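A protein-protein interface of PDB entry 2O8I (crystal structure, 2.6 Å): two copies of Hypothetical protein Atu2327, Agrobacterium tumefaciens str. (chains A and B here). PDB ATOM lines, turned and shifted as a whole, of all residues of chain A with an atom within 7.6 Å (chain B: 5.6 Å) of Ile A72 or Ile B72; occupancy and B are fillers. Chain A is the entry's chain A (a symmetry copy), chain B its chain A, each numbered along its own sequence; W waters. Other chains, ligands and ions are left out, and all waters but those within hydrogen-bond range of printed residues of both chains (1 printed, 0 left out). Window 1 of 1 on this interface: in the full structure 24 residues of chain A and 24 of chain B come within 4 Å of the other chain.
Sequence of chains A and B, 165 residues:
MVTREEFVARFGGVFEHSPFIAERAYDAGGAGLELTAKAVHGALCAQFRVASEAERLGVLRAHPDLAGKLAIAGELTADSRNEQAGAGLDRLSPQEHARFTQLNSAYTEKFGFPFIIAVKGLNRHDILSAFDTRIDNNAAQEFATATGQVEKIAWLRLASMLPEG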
ATOM      1  N   GLY A  13      21.129  11.228  10.534  1.00  0.00           N
ATOM      2  CA  GLY A  13      20.382  12.148  11.371  1.00  0.00           C
ATOM      3  C   GLY A  13      19.065  12.639  10.788  1.00  0.00           C
ATOM      4  O   GLY A  13      18.355  13.413  11.428  1.00  0.00           O
ATOM      5  N   GLU A  16      15.962  11.738  13.332  1.00  0.00           N
ATOM      6  CA  GLU A  16      16.785  12.112  14.430  1.00  0.00           C
ATOM      7  C   GLU A  16      17.218  10.915  15.274  1.00  0.00           C
ATOM      8  O   GLU A  16      16.406  10.066  15.572  1.00  0.00           O
ATOM      9  CB  GLU A  16      16.024  13.135  15.262  1.00  0.00           C
ATOM     10  CG  GLU A  16      16.936  13.873  16.168  1.00  0.00           C
ATOM     11  CD  GLU A  16      17.410  15.158  15.561  1.00  0.00           C
ATOM     12  OE1 GLU A  16      16.846  15.596  14.561  1.00  0.00           O
ATOM     13  OE2 GLU A  16      18.316  15.757  16.105  1.00  0.00           O
ATOM     14  N   HIS A  63      12.807  12.106  18.579  1.00  0.00           N
ATOM     15  CA  HIS A  63      12.651  13.369  17.907  1.00  0.00           C
ATOM     16  C   HIS A  63      12.663  14.586  18.867  1.00  0.00           C
ATOM     17  O   HIS A  63      12.089  14.544  19.954  1.00  0.00           O
ATOM     18  CB  HIS A  63      11.380  13.336  17.093  1.00  0.00           C
ATOM     19  CG  HIS A  63      11.333  14.376  16.036  1.00  0.00           C
ATOM     20  ND1 HIS A  63      11.712  14.126  14.739  1.00  0.00           N
ATOM     21  CD2 HIS A  63      10.987  15.683  16.085  1.00  0.00           C
ATOM     22  CE1 HIS A  63      11.574  15.228  14.020  1.00  0.00           C
ATOM     23  NE2 HIS A  63      11.127  16.185  14.810  1.00  0.00           N
ATOM     24  N   PRO A  64      13.378  15.661  18.496  1.00  0.00           N
ATOM     25  CA  PRO A  64      13.409  16.811  19.404  1.00  0.00           C
ATOM     26  C   PRO A  64      12.064  17.520  19.517  1.00  0.00           C
ATOM     27  O   PRO A  64      11.263  17.537  18.549  1.00  0.00           O
ATOM     28  CB  PRO A  64      14.427  17.758  18.757  1.00  0.00           C
ATOM     29  CG  PRO A  64      14.523  17.332  17.346  1.00  0.00           C
ATOM     30  CD  PRO A  64      14.241  15.858  17.311  1.00  0.00           C
ATOM     31  N   ASP A  65      11.829  18.098  20.693  1.00  0.00           N
ATOM     32  CA  ASP A  65      10.650  18.920  20.900  1.00  0.00           C
ATOM     33  C   ASP A  65      10.816  20.307  20.261  1.00  0.00           C
ATOM     34  O   ASP A  65      11.924  20.752  19.918  1.00  0.00           O
ATOM     35  CB  ASP A  65      10.284  19.008  22.386  1.00  0.00           C
ATOM     36  CG  ASP A  65      11.400  19.571  23.230  1.00  0.00           C
ATOM     37  OD1 ASP A  65      12.311  20.252  22.743  1.00  0.00           O
ATOM     38  OD2 ASP A  65      11.367  19.350  24.430  1.00  0.00           O
ATOM     39  N   LEU A  66       9.689  20.964  20.082  1.00  0.00           N
ATOM     40  CA  LEU A  66       9.655  22.239  19.455  1.00  0.00           C
ATOM     41  C   LEU A  66      10.617  23.295  20.071  1.00  0.00           C
ATOM     42  O   LEU A  66      11.406  23.939  19.366  1.00  0.00           O
ATOM     43  CB  LEU A  66       8.213  22.683  19.505  1.00  0.00           C
ATOM     44  CG  LEU A  66       7.847  23.747  18.504  1.00  0.00           C
ATOM     45  CD1 LEU A  66       8.541  23.522  17.218  1.00  0.00           C
ATOM     46  CD2 LEU A  66       6.376  23.601  18.352  1.00  0.00           C
ATOM     47  N   ALA A  67      10.589  23.464  21.379  1.00  0.00           N
ATOM     48  CA  ALA A  67      11.521  24.429  22.024  1.00  0.00           C
ATOM     49  C   ALA A  67      12.969  24.143  21.699  1.00  0.00           C
ATOM     50  O   ALA A  67      13.740  25.067  21.438  1.00  0.00           O
ATOM     51  CB  ALA A  67      11.310  24.480  23.477  1.00  0.00           C
ATOM     52  N   GLY A  68      13.339  22.874  21.667  1.00  0.00           N
ATOM     53  CA  GLY A  68      14.670  22.470  21.266  1.00  0.00           C
ATOM     54  C   GLY A  68      14.976  22.848  19.827  1.00  0.00           C
ATOM     55  O   GLY A  68      16.128  23.187  19.507  1.00  0.00           O
ATOM     56  N   LYS A  69      13.984  22.792  18.931  1.00  0.00           N
ATOM     57  CA  LYS A  69      14.263  23.179  17.558  1.00  0.00           C
ATOM     58  C   LYS A  69      14.445  24.696  17.491  1.00  0.00           C
ATOM     59  O   LYS A  69      15.337  25.196  16.793  1.00  0.00           O
ATOM     60  CB  LYS A  69      13.181  22.713  16.583  1.00  0.00           C
ATOM     61  CG  LYS A  69      13.031  21.213  16.469  1.00  0.00           C
ATOM     62  CD  LYS A  69      11.931  20.800  15.433  1.00  0.00           C
ATOM     63  CE  LYS A  69      12.134  19.321  15.004  1.00  0.00           C
ATOM     64  NZ  LYS A  69      11.057  18.842  14.063  1.00  0.00           N
ATOM     65  N   LEU A  70      13.600  25.423  18.214  1.00  0.00           N
ATOM     66  CA  LEU A  70      13.652  26.886  18.202  1.00  0.00           C
ATOM     67  C   LEU A  70      14.988  27.393  18.746  1.00  0.00           C
ATOM     68  O   LEU A  70      15.584  28.335  18.205  1.00  0.00           O
ATOM     69  CB  LEU A  70      12.466  27.472  18.979  1.00  0.00           C
ATOM     70  CG  LEU A  70      11.118  27.182  18.285  1.00  0.00           C
ATOM     71  CD1 LEU A  70       9.993  27.622  19.158  1.00  0.00           C
ATOM     72  CD2 LEU A  70      11.003  27.924  16.983  1.00  0.00           C
ATOM     73  N   ALA A  71      15.475  26.734  19.790  1.00  0.00           N
ATOM     74  CA  ALA A  71      16.762  27.095  20.345  1.00  0.00           C
ATOM     75  C   ALA A  71      17.925  26.826  19.389  1.00  0.00           C
ATOM     76  O   ALA A  71      18.853  27.619  19.278  1.00  0.00           O
ATOM     77  CB  ALA A  71      16.978  26.398  21.662  1.00  0.00           C
ATOM     78  N   ILE A  72      17.877  25.721  18.671  1.00  0.00           N
ATOM     79  CA  ILE A  72      18.899  25.527  17.655  1.00  0.00           C
ATOM     80  C   ILE A  72      18.835  26.609  16.559  1.00  0.00           C
ATOM     81  O   ILE A  72      19.879  27.123  16.143  1.00  0.00           O
ATOM     82  CB  ILE A  72      18.912  24.095  17.104  1.00  0.00           C
ATOM     83  CG1 ILE A  72      19.651  23.184  18.097  1.00  0.00           C
ATOM     84  CG2 ILE A  72      19.636  24.053  15.790  1.00  0.00           C
ATOM     85  CD1 ILE A  72      18.958  21.857  18.404  1.00  0.00           C
ATOM     86  N   ALA A  73      17.627  26.987  16.141  1.00  0.00           N
ATOM     87  CA  ALA A  73      17.463  28.108  15.224  1.00  0.00           C
ATOM     88  C   ALA A  73      18.041  29.438  15.799  1.00  0.00           C
ATOM     89  O   ALA A  73      18.804  30.140  15.120  1.00  0.00           O
ATOM     90  CB  ALA A  73      16.007  28.257  14.817  1.00  0.00           C
ATOM     91  N   GLY A  74      17.701  29.771  17.040  1.00  0.00           N
ATOM     92  CA  GLY A  74      18.330  30.904  17.735  1.00  0.00           C
ATOM     93  C   GLY A  74      19.851  30.981  17.730  1.00  0.00           C
ATOM     94  O   GLY A  74      20.411  32.055  17.908  1.00  0.00           O
ATOM     95  N   GLU A  75      20.528  29.845  17.542  1.00  0.00           N
ATOM     96  CA  GLU A  75      21.990  29.831  17.386  1.00  0.00           C
ATOM     97  C   GLU A  75      22.457  30.289  16.046  1.00  0.00           C
ATOM     98  O   GLU A  75      23.616  30.648  15.921  1.00  0.00           O
ATOM     99  CB  GLU A  75      22.567  28.439  17.484  1.00  0.00           C
ATOM    100  CG  GLU A  75      22.559  27.803  18.812  1.00  0.00           C
ATOM    101  CD  GLU A  75      23.113  26.406  18.704  1.00  0.00           C
ATOM    102  OE1 GLU A  75      24.292  26.273  18.228  1.00  0.00           O
ATOM    103  OE2 GLU A  75      22.341  25.473  19.077  1.00  0.00           O
ATOM    104  N   LEU A  76      21.603  30.222  15.034  1.00  0.00           N
ATOM    105  CA  LEU A  76      22.058  30.530  13.690  1.00  0.00           C
ATOM    106  C   LEU A  76      21.494  31.834  13.135  1.00  0.00           C
ATOM    107  O   LEU A  76      22.213  32.571  12.468  1.00  0.00           O
ATOM    108  CB  LEU A  76      21.779  29.360  12.735  1.00  0.00           C
ATOM    109  CG  LEU A  76      21.747  27.849  13.139  1.00  0.00           C
ATOM    110  CD1 LEU A  76      21.905  26.917  11.913  1.00  0.00           C
ATOM    111  CD2 LEU A  76      22.775  27.381  14.195  1.00  0.00           C
ATOM    112  N   THR A  77      20.223  32.127  13.442  1.00  0.00           N
ATOM    113  CA  THR A  77      19.444  33.242  12.822  1.00  0.00           C
ATOM    114  C   THR A  77      19.934  34.661  13.192  1.00  0.00           C
ATOM    115  O   THR A  77      20.936  35.149  12.670  1.00  0.00           O
ATOM    116  CB  THR A  77      17.915  33.074  13.125  1.00  0.00           C
ATOM    117  N   VAL A 119       7.198  22.616  10.629  1.00  0.00           N
ATOM    118  CA  VAL A 119       6.994  23.969  11.071  1.00  0.00           C
ATOM    119  C   VAL A 119       7.297  25.001   9.957  1.00  0.00           C
ATOM    120  O   VAL A 119       6.969  26.190  10.112  1.00  0.00           O
ATOM    121  CB  VAL A 119       7.872  24.138  12.342  1.00  0.00           C
ATOM    122  CG1 VAL A 119       8.732  25.384  12.315  1.00  0.00           C
ATOM    123  CG2 VAL A 119       7.056  23.930  13.605  1.00  0.00           C
ATOM    124  N   LYS A 120       7.891  24.560   8.840  1.00  0.00           N
ATOM    125  CA  LYS A 120       8.151  25.455   7.707  1.00  0.00           C
ATOM    126  C   LYS A 120       6.871  26.198   7.325  1.00  0.00           C
ATOM    127  O   LYS A 120       5.829  25.584   7.111  1.00  0.00           O
ATOM    128  CB  LYS A 120       8.765  24.726   6.487  1.00  0.00           C
ATOM    129  CG  LYS A 120       8.895  25.618   5.244  1.00  0.00           C
ATOM    130  CD  LYS A 120      10.063  25.303   4.245  1.00  0.00           C
ATOM    131  CE  LYS A 120      11.495  25.274   4.872  1.00  0.00           C
ATOM    132  NZ  LYS A 120      11.840  26.486   5.701  1.00  0.00           N
ATOM    133  N   ILE A 153       9.267  16.158   8.133  1.00  0.00           N
ATOM    134  CA  ILE A 153      10.461  16.795   8.553  1.00  0.00           C
ATOM    135  C   ILE A 153      11.677  16.216   7.773  1.00  0.00           C
ATOM    136  O   ILE A 153      12.571  16.969   7.334  1.00  0.00           O
ATOM    137  CB  ILE A 153      10.549  16.670  10.045  1.00  0.00           C
ATOM    138  CG1 ILE A 153       9.442  17.570  10.640  1.00  0.00           C
ATOM    139  CG2 ILE A 153      11.942  17.050  10.502  1.00  0.00           C
ATOM    140  CD1 ILE A 153       8.935  17.203  12.049  1.00  0.00           C
ATOM    141  N   ARG A 157      14.293  18.415   5.779  1.00  0.00           N
ATOM    142  CA  ARG A 157      15.737  18.346   6.034  1.00  0.00           C
ATOM    143  C   ARG A 157      16.516  18.064   4.761  1.00  0.00           C
ATOM    144  O   ARG A 157      17.383  18.876   4.378  1.00  0.00           O
ATOM    145  CB  ARG A 157      16.056  17.345   7.131  1.00  0.00           C
ATOM    146  CG  ARG A 157      15.484  17.835   8.457  1.00  0.00           C
ATOM    147  CD  ARG A 157      15.505  16.754   9.473  1.00  0.00           C
ATOM    148  NE  ARG A 157      15.289  17.307  10.793  1.00  0.00           N
ATOM    149  CZ  ARG A 157      15.546  16.659  11.921  1.00  0.00           C
ATOM    150  NH1 ARG A 157      16.070  15.434  11.868  1.00  0.00           N
ATOM    151  NH2 ARG A 157      15.292  17.240  13.096  1.00  0.00           N
ATOM    152  N   SER A 160      16.908  20.798   2.188  1.00  0.00           N
ATOM    153  CA  SER A 160      17.917  21.844   2.417  1.00  0.00           C
ATOM    154  C   SER A 160      19.334  21.380   2.033  1.00  0.00           C
ATOM    155  O   SER A 160      20.195  22.210   1.737  1.00  0.00           O
ATOM    156  CB  SER A 160      17.896  22.373   3.857  1.00  0.00           C
ATOM    157  OG  SER A 160      18.220  21.342   4.790  1.00  0.00           O
ATOM    158  N   MET A 161      19.550  20.067   2.028  1.00  0.00           N
ATOM    159  CA  MET A 161      20.843  19.482   1.786  1.00  0.00           C
ATOM    160  C   MET A 161      21.093  19.040   0.351  1.00  0.00           C
ATOM    161  O   MET A 161      22.224  18.747   0.006  1.00  0.00           O
ATOM    162  CB  MET A 161      20.958  18.211   2.570  1.00  0.00           C
ATOM    163  CG  MET A 161      21.281  18.307   4.007  1.00  0.00           C
ATOM    164  SD  MET A 161      20.825  16.484   4.670  1.00  0.00           S
ATOM    165  CE  MET A 161      19.273  16.889   5.785  1.00  0.00           C
ATOM    166  N   GLU B  16      22.546  20.276  25.540  1.00  0.00           N
ATOM    167  CA  GLU B  16      21.827  19.283  24.818  1.00  0.00           C
ATOM    168  C   GLU B  16      21.828  17.928  25.525  1.00  0.00           C
ATOM    169  O   GLU B  16      22.856  17.501  26.003  1.00  0.00           O
ATOM    170  CB  GLU B  16      22.432  19.184  23.424  1.00  0.00           C
ATOM    171  CG  GLU B  16      21.512  18.492  22.489  1.00  0.00           C
ATOM    172  CD  GLU B  16      20.656  19.458  21.729  1.00  0.00           C
ATOM    173  OE1 GLU B  16      20.944  20.653  21.736  1.00  0.00           O
ATOM    174  OE2 GLU B  16      19.722  19.023  21.085  1.00  0.00           O
ATOM    175  N   PRO B  64      24.833  18.102  19.313  1.00  0.00           N
ATOM    176  CA  PRO B  64      24.659  17.799  17.889  1.00  0.00           C
ATOM    177  C   PRO B  64      25.793  18.333  17.021  1.00  0.00           C
ATOM    178  O   PRO B  64      26.413  19.376  17.344  1.00  0.00           O
ATOM    179  CB  PRO B  64      23.357  18.522  17.521  1.00  0.00           C
ATOM    180  CG  PRO B  64      23.160  19.542  18.571  1.00  0.00           C
ATOM    181  CD  PRO B  64      23.782  19.007  19.827  1.00  0.00           C
ATOM    182  N   ALA B  67      26.039  19.630  10.757  1.00  0.00           N
ATOM    183  CA  ALA B  67      25.006  19.258   9.752  1.00  0.00           C
ATOM    184  C   ALA B  67      23.639  19.066  10.367  1.00  0.00           C
ATOM    185  O   ALA B  67      22.637  19.503   9.801  1.00  0.00           O
ATOM    186  CB  ALA B  67      25.410  18.067   8.992  1.00  0.00           C
ATOM    187  N   GLY B  68      23.588  18.458  11.541  1.00  0.00           N
ATOM    188  CA  GLY B  68      22.350  18.310  12.277  1.00  0.00           C
ATOM    189  C   GLY B  68      21.753  19.649  12.672  1.00  0.00           C
ATOM    190  O   GLY B  68      20.519  19.793  12.698  1.00  0.00           O
ATOM    191  N   LYS B  69      22.585  20.644  12.997  1.00  0.00           N
ATOM    192  CA  LYS B  69      22.022  21.937  13.349  1.00  0.00           C
ATOM    193  C   LYS B  69      21.468  22.604  12.088  1.00  0.00           C
ATOM    194  O   LYS B  69      20.389  23.210  12.114  1.00  0.00           O
ATOM    195  CB  LYS B  69      23.028  22.847  14.054  1.00  0.00           C
ATOM    196  CG  LYS B  69      23.519  22.337  15.390  1.00  0.00           C
ATOM    197  CD  LYS B  69      24.521  23.327  16.075  1.00  0.00           C
ATOM    198  CE  LYS B  69      24.622  23.014  17.593  1.00  0.00           C
ATOM    199  NZ  LYS B  69      25.632  23.888  18.294  1.00  0.00           N
ATOM    200  N   LEU B  70      22.209  22.493  10.991  1.00  0.00           N
ATOM    201  CA  LEU B  70      21.803  23.120   9.732  1.00  0.00           C
ATOM    202  C   LEU B  70      20.479  22.541   9.232  1.00  0.00           C
ATOM    203  O   LEU B  70      19.599  23.273   8.756  1.00  0.00           O
ATOM    204  CB  LEU B  70      22.912  22.985   8.681  1.00  0.00           C
ATOM    205  CG  LEU B  70      24.172  23.790   9.061  1.00  0.00           C
ATOM    206  CD1 LEU B  70      25.273  23.494   8.101  1.00  0.00           C
ATOM    207  CD2 LEU B  70      23.910  25.270   9.014  1.00  0.00           C
ATOM    208  N   ALA B  71      20.326  21.232   9.385  1.00  0.00           N
ATOM    209  CA  ALA B  71      19.086  20.592   8.998  1.00  0.00           C
ATOM    210  C   ALA B  71      17.895  21.025   9.855  1.00  0.00           C
ATOM    211  O   ALA B  71      16.796  21.238   9.354  1.00  0.00           O
ATOM    212  CB  ALA B  71      19.242  19.095   9.016  1.00  0.00           C
ATOM    213  N   ILE B  72      18.103  21.185  11.147  1.00  0.00           N
ATOM    214  CA  ILE B  72      17.021  21.737  11.945  1.00  0.00           C
ATOM    215  C   ILE B  72      16.657  23.171  11.512  1.00  0.00           C
ATOM    216  O   ILE B  72      15.470  23.501  11.416  1.00  0.00           O
ATOM    217  CB  ILE B  72      17.274  21.597  13.452  1.00  0.00           C
ATOM    218  CG1 ILE B  72      16.934  20.163  13.886  1.00  0.00           C
ATOM    219  CG2 ILE B  72      16.397  22.545  14.215  1.00  0.00           C
ATOM    220  CD1 ILE B  72      17.966  19.493  14.792  1.00  0.00           C
ATOM    221  N   ALA B  73      17.663  23.991  11.202  1.00  0.00           N
ATOM    222  CA  ALA B  73      17.412  25.311  10.636  1.00  0.00           C
ATOM    223  C   ALA B  73      16.621  25.243   9.294  1.00  0.00           C
ATOM    224  O   ALA B  73      15.618  25.950   9.116  1.00  0.00           O
ATOM    225  CB  ALA B  73      18.712  26.082  10.484  1.00  0.00           C
ATOM    226  N   GLY B  74      17.048  24.389   8.369  1.00  0.00           N
ATOM    227  CA  GLY B  74      16.273  24.121   7.149  1.00  0.00           C
ATOM    228  C   GLY B  74      14.795  23.788   7.310  1.00  0.00           C
ATOM    229  O   GLY B  74      14.024  23.960   6.374  1.00  0.00           O
ATOM    230  N   GLU B  75      14.394  23.298   8.486  1.00  0.00           N
ATOM    231  CA  GLU B  75      12.973  23.074   8.787  1.00  0.00           C
ATOM    232  C   GLU B  75      12.216  24.322   9.089  1.00  0.00           C
ATOM    233  O   GLU B  75      10.999  24.304   9.008  1.00  0.00           O
ATOM    234  CB  GLU B  75      12.772  22.250  10.036  1.00  0.00           C
ATOM    235  CG  GLU B  75      13.130  20.823   9.962  1.00  0.00           C
ATOM    236  CD  GLU B  75      12.922  20.181  11.309  1.00  0.00           C
ATOM    237  OE1 GLU B  75      11.753  20.252  11.823  1.00  0.00           O
ATOM    238  OE2 GLU B  75      13.943  19.642  11.830  1.00  0.00           O
ATOM    239  N   LEU B  76      12.902  25.381   9.499  1.00  0.00           N
ATOM    240  CA  LEU B  76      12.192  26.571   9.932  1.00  0.00           C
ATOM    241  C   LEU B  76      12.335  27.752   8.976  1.00  0.00           C
ATOM    242  O   LEU B  76      11.368  28.474   8.756  1.00  0.00           O
ATOM    243  CB  LEU B  76      12.603  26.965  11.358  1.00  0.00           C
ATOM    244  CG  LEU B  76      13.060  25.973  12.477  1.00  0.00           C
ATOM    245  CD1 LEU B  76      12.954  26.599  13.887  1.00  0.00           C
ATOM    246  CD2 LEU B  76      12.344  24.603  12.537  1.00  0.00           C
ATOM    247  N   ARG B 157      21.412  30.120  23.049  1.00  0.00           N
ATOM    248  CA  ARG B 157      20.080  29.519  23.202  1.00  0.00           C
ATOM    249  C   ARG B 157      19.214  30.315  24.162  1.00  0.00           C
ATOM    250  O   ARG B 157      18.130  30.787  23.765  1.00  0.00           O
ATOM    251  CB  ARG B 157      20.180  28.057  23.601  1.00  0.00           C
ATOM    252  CG  ARG B 157      20.805  27.254  22.467  1.00  0.00           C
ATOM    253  CD  ARG B 157      21.197  25.900  22.930  1.00  0.00           C
ATOM    254  NE  ARG B 157      21.465  25.044  21.795  1.00  0.00           N
ATOM    255  CZ  ARG B 157      21.542  23.722  21.865  1.00  0.00           C
ATOM    256  NH1 ARG B 157      21.329  23.113  23.033  1.00  0.00           N
ATOM    257  NH2 ARG B 157      21.818  23.011  20.768  1.00  0.00           N
HETATM  258  O   HOH W   1       9.610  21.476  11.244  1.00  0.00           O
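The guanidinium group (NE) of Arg B157 lies within salt-bridge range of the side-chain carboxylate (OE2) of Glu A75, at 2.9 Å.
The backbone carbonyl oxygen (O) of Gly B74 lies close to the side-chain amino group (NZ) of Lys A120 (3.4 Å).
The guanidinium group of Arg A157 is in salt-bridge range of the side-chain carboxylate of Glu B75 (2.9 Å).
NZ of Lys B69 is in salt-bridge range of OE1 of Glu A75 (2.7 Å).
O of Glu B75 sits at hydrogen-bond distance from N of Lys A120.
OE1 of Glu B75 lies within salt-bridge range of NZ of Lys A69 (2.7 Å).
NH2 of Arg A157 lies within salt-bridge range of OE1 of Glu A16 (2.7 Å).
O of Gly A13 is in hydrogen-bond range of NH1 of Arg A157 (3.1 Å).
O of Arg A157 lies within hydrogen-bond range of OG of Ser A160, 2.6 Å away.
OE1 of Glu B16 lies within salt-bridge range of NH2 of Arg B157.
The side-chain amino group of Lys A69 lies within hydrogen-bond range of a ring nitrogen (NE2) of His A63 (2.8 Å).
OE2 of Glu A16 touches CD1 of Ile B72, 3.98 Å away.
CD2 of Leu A70 touches CD1 of Leu B76, at 3.9 Å.
Ile A72 touches Glu B16.
Ile A72 touches Ile B72 (CG2 to CG2, 3.9 Å).
Leu A76 touches Leu B70.
C of Leu B76 touches NZ of Lys A120, 3.5 Å away.
CG2 of Ile A153 touches CD of Glu B75 (3.4 Å).
Ala B71 touches Arg A157 (O to CG, 3.8 Å).
Ile B72 touches Arg A157.
Ala B71 touches Met A161.
Of the printed residues of chain B, Lys A69 touches Ile B72 (3.8 Å) and Glu B75 (2.7 Å).
Ile A72 touches just these residues of chain B: Glu B16, Lys B69, Ile B72 and Arg B157.
Printed residues of chain B within 4 Å of Glu A75: Lys B69 and Arg B157.
Of the printed residues of chain B, Met A161 touches Ala B71 (3.9 Å).
Of the printed residues of chain A, Ala B71 touches Arg A157 and Met A161.
The nearest residue of chain B that does not touch Ile A72 is Pro B64 (4.8 Å).
The nearest residue of chain A that does not touch Ile B72 is Pro A64 (4.8 Å).
The nearest printed residue of chain A that does not touch Ala B73 is Ile A72 (5.0 Å).
Of the 13 printed residues of chain B, 10 touch a printed residue of chain A.
Hydrophobic or aromatic side chains of chain B within 4 Å of the printed part of chain A: Leu B70, Ala B71, Ile B72, Ala B73 and Leu B76.
Along chain B the printed residues that touch a printed residue of chain A span positions 16 to 157.
Hydrophobic or aromatic side chains of chain A that line the printed part of chain B: Leu A70, Ile A72, Ala A73, Leu A76, Val A119, Ile A153 and Met A161.
Among the printed residues, 24 pairs touch across the chains.
Among the printed residues, Asp or Glu carboxylates within 4 Å of a Lys or Arg side-chain nitrogen of the other chain: Lys A69 with Glu B75 (2.7 Å), Glu A75 with Lys B69 (2.7 Å), Glu A75 with Arg B157 (2.9 Å) and Arg A157 with Glu B75 (2.9 Å).
Glu A16 touches Ile B72, and with the chains exchanged Ile A72 touches Glu B16.
Ile B72 touches its own counterpart, Ile A72.
Ala A73 touches Leu B76, and with the chains exchanged Leu A76 touches Ala B73.
Glu A75 touches Arg B157, and with the chains exchanged Arg A157 touches Glu B75.
Positions printed for both chains: 16, 64, 67, 68, 69, 70, 71, 72, 73, 74, 75, 76 and 157.
Of the 24 pairs that touch across the chains among the printed residues, 17 have their exchanged pair printed and touching as well.
Water W1 lies within hydrogen-bond range of OE1 of Glu B75 and N of Val A119.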
